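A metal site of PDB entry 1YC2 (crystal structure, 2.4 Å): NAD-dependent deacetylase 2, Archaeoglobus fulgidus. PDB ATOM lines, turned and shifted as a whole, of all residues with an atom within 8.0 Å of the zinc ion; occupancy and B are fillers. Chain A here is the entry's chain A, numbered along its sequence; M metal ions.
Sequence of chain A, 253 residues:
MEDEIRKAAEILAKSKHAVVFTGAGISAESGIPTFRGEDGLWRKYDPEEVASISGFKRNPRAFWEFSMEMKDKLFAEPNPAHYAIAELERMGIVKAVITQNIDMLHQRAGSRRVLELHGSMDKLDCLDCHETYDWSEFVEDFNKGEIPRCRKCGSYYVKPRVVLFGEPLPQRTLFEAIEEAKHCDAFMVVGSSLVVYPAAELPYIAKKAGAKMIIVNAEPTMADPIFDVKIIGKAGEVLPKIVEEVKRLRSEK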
ATOM      1  N   LYS A  16      27.802  -4.126  21.974  1.00  0.00           N
ATOM      2  CA  LYS A  16      27.981  -3.309  20.780  1.00  0.00           C
ATOM      3  C   LYS A  16      26.816  -2.347  20.525  1.00  0.00           C
ATOM      4  O   LYS A  16      26.727  -1.744  19.455  1.00  0.00           O
ATOM      5  CB  LYS A  16      28.165  -4.222  19.557  1.00  0.00           C
ATOM      6  N   HIS A  17      25.931  -2.198  21.512  1.00  0.00           N
ATOM      7  CA  HIS A  17      24.799  -1.301  21.369  1.00  0.00           C
ATOM      8  C   HIS A  17      24.217  -0.938  22.722  1.00  0.00           C
ATOM      9  O   HIS A  17      23.045  -1.195  22.997  1.00  0.00           O
ATOM     10  CB  HIS A  17      23.730  -1.946  20.505  1.00  0.00           C
ATOM     11  CG  HIS A  17      22.798  -0.967  19.869  1.00  0.00           C
ATOM     12  ND1 HIS A  17      22.914  -0.566  18.556  1.00  0.00           N
ATOM     13  CD2 HIS A  17      21.748  -0.281  20.378  1.00  0.00           C
ATOM     14  CE1 HIS A  17      21.970   0.320  18.281  1.00  0.00           C
ATOM     15  NE2 HIS A  17      21.251   0.516  19.375  1.00  0.00           N
ATOM     16  N   ALA A  18      25.035  -0.338  23.585  1.00  0.00           N
ATOM     17  CA  ALA A  18      24.601   0.035  24.919  1.00  0.00           C
ATOM     18  C   ALA A  18      23.919   1.389  24.958  1.00  0.00           C
ATOM     19  O   ALA A  18      24.236   2.283  24.171  1.00  0.00           O
ATOM     20  CB  ALA A  18      25.790   0.045  25.846  1.00  0.00           C
ATOM     21  N   VAL A  19      22.965   1.537  25.880  1.00  0.00           N
ATOM     22  CA  VAL A  19      22.220   2.785  26.043  1.00  0.00           C
ATOM     23  C   VAL A  19      22.312   3.335  27.465  1.00  0.00           C
ATOM     24  O   VAL A  19      22.149   2.605  28.433  1.00  0.00           O
ATOM     25  CB  VAL A  19      20.739   2.586  25.674  1.00  0.00           C
ATOM     26  CG1 VAL A  19      19.940   3.826  26.000  1.00  0.00           C
ATOM     27  CG2 VAL A  19      20.624   2.272  24.185  1.00  0.00           C
ATOM     28  N   VAL A  94      28.504   2.716  23.454  1.00  0.00           N
ATOM     29  CA  VAL A  94      27.265   3.497  23.651  1.00  0.00           C
ATOM     30  C   VAL A  94      26.738   4.019  22.314  1.00  0.00           C
ATOM     31  O   VAL A  94      27.440   4.715  21.569  1.00  0.00           O
ATOM     32  CB  VAL A  94      27.521   4.689  24.611  1.00  0.00           C
ATOM     33  CG1 VAL A  94      26.352   5.668  24.549  1.00  0.00           C
ATOM     34  CG2 VAL A  94      27.706   4.170  26.026  1.00  0.00           C
ATOM     35  N   LYS A  95      25.489   3.673  22.012  1.00  0.00           N
ATOM     36  CA  LYS A  95      24.854   4.077  20.769  1.00  0.00           C
ATOM     37  C   LYS A  95      23.840   5.195  20.961  1.00  0.00           C
ATOM     38  O   LYS A  95      23.400   5.822  19.987  1.00  0.00           O
ATOM     39  CB  LYS A  95      24.159   2.866  20.123  1.00  0.00           C
ATOM     40  CG  LYS A  95      25.116   1.891  19.493  1.00  0.00           C
ATOM     41  CD  LYS A  95      25.827   2.530  18.322  1.00  0.00           C
ATOM     42  CE  LYS A  95      26.768   1.545  17.627  1.00  0.00           C
ATOM     43  NZ  LYS A  95      27.832   1.042  18.538  1.00  0.00           N
ATOM     44  N   ALA A  96      23.467   5.431  22.212  1.00  0.00           N
ATOM     45  CA  ALA A  96      22.503   6.486  22.488  1.00  0.00           C
ATOM     46  C   ALA A  96      22.480   6.880  23.943  1.00  0.00           C
ATOM     47  O   ALA A  96      22.782   6.080  24.821  1.00  0.00           O
ATOM     48  CB  ALA A  96      21.117   6.036  22.058  1.00  0.00           C
ATOM     49  N   ARG A 113      24.289  11.408  19.973  1.00  0.00           N
ATOM     50  CA  ARG A 113      22.882  11.022  19.966  1.00  0.00           C
ATOM     51  C   ARG A 113      22.291  11.170  21.356  1.00  0.00           C
ATOM     52  O   ARG A 113      22.530  10.358  22.252  1.00  0.00           O
ATOM     53  CB  ARG A 113      22.733   9.578  19.490  1.00  0.00           C
ATOM     54  CG  ARG A 113      21.295   9.080  19.461  1.00  0.00           C
ATOM     55  CD  ARG A 113      21.185   7.828  18.627  1.00  0.00           C
ATOM     56  NE  ARG A 113      19.842   7.252  18.632  1.00  0.00           N
ATOM     57  CZ  ARG A 113      18.774   7.830  18.106  1.00  0.00           C
ATOM     58  NH1 ARG A 113      17.597   7.223  18.159  1.00  0.00           N
ATOM     59  NH2 ARG A 113      18.868   9.023  17.534  1.00  0.00           N
ATOM     60  N   LEU A 115      18.665  11.844  23.296  1.00  0.00           N
ATOM     61  CA  LEU A 115      17.210  11.888  23.271  1.00  0.00           C
ATOM     62  C   LEU A 115      16.783  12.657  24.519  1.00  0.00           C
ATOM     63  O   LEU A 115      16.941  12.165  25.629  1.00  0.00           O
ATOM     64  CB  LEU A 115      16.667  10.450  23.262  1.00  0.00           C
ATOM     65  CG  LEU A 115      17.148   9.613  22.040  1.00  0.00           C
ATOM     66  CD1 LEU A 115      16.535   8.214  22.065  1.00  0.00           C
ATOM     67  CD2 LEU A 115      16.755  10.324  20.745  1.00  0.00           C
ATOM     68  N   GLU A 176      11.396   7.057  20.222  1.00  0.00           N
ATOM     69  CA  GLU A 176      12.743   6.620  19.912  1.00  0.00           C
ATOM     70  C   GLU A 176      13.444   6.034  21.146  1.00  0.00           C
ATOM     71  O   GLU A 176      14.215   5.074  21.028  1.00  0.00           O
ATOM     72  CB  GLU A 176      13.574   7.797  19.401  1.00  0.00           C
ATOM     73  CG  GLU A 176      13.639   7.964  17.902  1.00  0.00           C
ATOM     74  CD  GLU A 176      14.554   9.120  17.512  1.00  0.00           C
ATOM     75  OE1 GLU A 176      14.206  10.285  17.828  1.00  0.00           O
ATOM     76  OE2 GLU A 176      15.626   8.871  16.898  1.00  0.00           O
ATOM     77  N   ALA A 177      13.193   6.619  22.317  1.00  0.00           N
ATOM     78  CA  ALA A 177      13.835   6.153  23.544  1.00  0.00           C
ATOM     79  C   ALA A 177      13.354   4.741  23.906  1.00  0.00           C
ATOM     80  O   ALA A 177      14.159   3.874  24.273  1.00  0.00           O
ATOM     81  CB  ALA A 177      13.547   7.119  24.701  1.00  0.00           C
ATOM     82  N   GLU A 179      12.069   2.551  21.848  1.00  0.00           N
ATOM     83  CA  GLU A 179      12.605   1.625  20.867  1.00  0.00           C
ATOM     84  C   GLU A 179      14.048   1.281  21.240  1.00  0.00           C
ATOM     85  O   GLU A 179      14.499   0.136  21.110  1.00  0.00           O
ATOM     86  CB  GLU A 179      12.552   2.238  19.467  1.00  0.00           C
ATOM     87  CG  GLU A 179      13.375   1.464  18.440  1.00  0.00           C
ATOM     88  CD  GLU A 179      13.026  -0.015  18.404  1.00  0.00           C
ATOM     89  OE1 GLU A 179      13.811  -0.799  17.820  1.00  0.00           O
ATOM     90  OE2 GLU A 179      11.956  -0.400  18.943  1.00  0.00           O
ATOM     91  N   GLU A 180      14.757   2.307  21.733  1.00  0.00           N
ATOM     92  CA  GLU A 180      16.145   2.191  22.157  1.00  0.00           C
ATOM     93  C   GLU A 180      16.231   1.160  23.284  1.00  0.00           C
ATOM     94  O   GLU A 180      17.057   0.241  23.258  1.00  0.00           O
ATOM     95  CB  GLU A 180      16.602   3.571  22.641  1.00  0.00           C
ATOM     96  CG  GLU A 180      18.087   3.852  22.547  1.00  0.00           C
ATOM     97  CD  GLU A 180      18.657   3.566  21.167  1.00  0.00           C
ATOM     98  OE1 GLU A 180      18.951   2.386  20.922  1.00  0.00           O
ATOM     99  OE2 GLU A 180      18.799   4.511  20.350  1.00  0.00           O
ATOM    100  N   ALA A 181      15.362   1.283  24.276  1.00  0.00           N
ATOM    101  CA  ALA A 181      15.362   0.355  25.391  1.00  0.00           C
ATOM    102  C   ALA A 181      15.049  -1.091  24.951  1.00  0.00           C
ATOM    103  O   ALA A 181      15.540  -2.039  25.549  1.00  0.00           O
ATOM    104  CB  ALA A 181      14.356   0.791  26.432  1.00  0.00           C
ATOM    105  N   LYS A 182      14.260  -1.241  23.881  1.00  0.00           N
ATOM    106  CA  LYS A 182      13.876  -2.574  23.391  1.00  0.00           C
ATOM    107  C   LYS A 182      14.909  -3.294  22.552  1.00  0.00           C
ATOM    108  O   LYS A 182      14.845  -4.513  22.414  1.00  0.00           O
ATOM    109  CB  LYS A 182      12.579  -2.494  22.579  1.00  0.00           C
ATOM    110  CG  LYS A 182      11.341  -2.253  23.393  1.00  0.00           C
ATOM    111  CD  LYS A 182      10.091  -2.313  22.515  1.00  0.00           C
ATOM    112  CE  LYS A 182       8.805  -2.135  23.331  1.00  0.00           C
ATOM    113  NZ  LYS A 182       7.580  -2.288  22.494  1.00  0.00           N
ATOM    114  N   HIS A 183      15.864  -2.568  21.974  1.00  0.00           N
ATOM    115  CA  HIS A 183      16.832  -3.249  21.150  1.00  0.00           C
ATOM    116  C   HIS A 183      18.280  -3.103  21.586  1.00  0.00           C
ATOM    117  O   HIS A 183      19.180  -3.582  20.902  1.00  0.00           O
ATOM    118  CB  HIS A 183      16.653  -2.836  19.679  1.00  0.00           C
ATOM    119  CG  HIS A 183      17.131  -1.443  19.347  1.00  0.00           C
ATOM    120  ND1 HIS A 183      16.432  -0.605  18.513  1.00  0.00           N
ATOM    121  CD2 HIS A 183      18.266  -0.789  19.693  1.00  0.00           C
ATOM    122  CE1 HIS A 183      17.123   0.511  18.342  1.00  0.00           C
ATOM    123  NE2 HIS A 183      18.234   0.431  19.041  1.00  0.00           N
ATOM    124  N   CYS A 184      18.515  -2.464  22.728  1.00  0.00           N
ATOM    125  CA  CYS A 184      19.873  -2.311  23.236  1.00  0.00           C
ATOM    126  C   CYS A 184      20.322  -3.635  23.871  1.00  0.00           C
ATOM    127  O   CYS A 184      19.491  -4.493  24.165  1.00  0.00           O
ATOM    128  CB  CYS A 184      19.940  -1.185  24.270  1.00  0.00           C
ATOM    129  SG  CYS A 184      19.060  -1.549  25.823  1.00  0.00           S
ATOM    130  N   ASP A 185      21.631  -3.807  24.085  1.00  0.00           N
ATOM    131  CA  ASP A 185      22.134  -5.029  24.697  1.00  0.00           C
ATOM    132  C   ASP A 185      22.701  -4.757  26.082  1.00  0.00           C
ATOM    133  O   ASP A 185      23.108  -5.671  26.794  1.00  0.00           O
ATOM    134  CB  ASP A 185      23.166  -5.725  23.785  1.00  0.00           C
ATOM    135  CG  ASP A 185      24.372  -4.846  23.482  1.00  0.00           C
ATOM    136  OD1 ASP A 185      24.343  -3.633  23.774  1.00  0.00           O
ATOM    137  OD2 ASP A 185      25.363  -5.384  22.933  1.00  0.00           O
HETATM  138 ZN    ZN M   1      19.759   2.047  19.167  1.00  0.00          ZN
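Three residues have an atom within 4 Å of the zinc ion: His 17, Glu 180 and His 183.
The zinc ion is bound by the side-chain carboxylate of Glu 180 (2.0 Å), a ring nitrogen (NE2) of His 17 (2.1 Å) and a ring nitrogen (NE2) of His 183 (2.2 Å).
ND1 of His 183 is in hydrogen-bond range of OE1 of Glu 179, at 2.7 Å. The backbone NH (N) of His 17 sits close to the side-chain carboxylate (OD1) of Asp 185, at 3.1 Å. The side-chain sulfur (SG) of Cys 184 sits close to the backbone carbonyl oxygen (O) of Glu 180, 3.7 Å away. The guanidinium group (NE) of Arg 113 lies within salt-bridge range of the side-chain carboxylate (OE2) of Glu 180 (3.4 Å).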
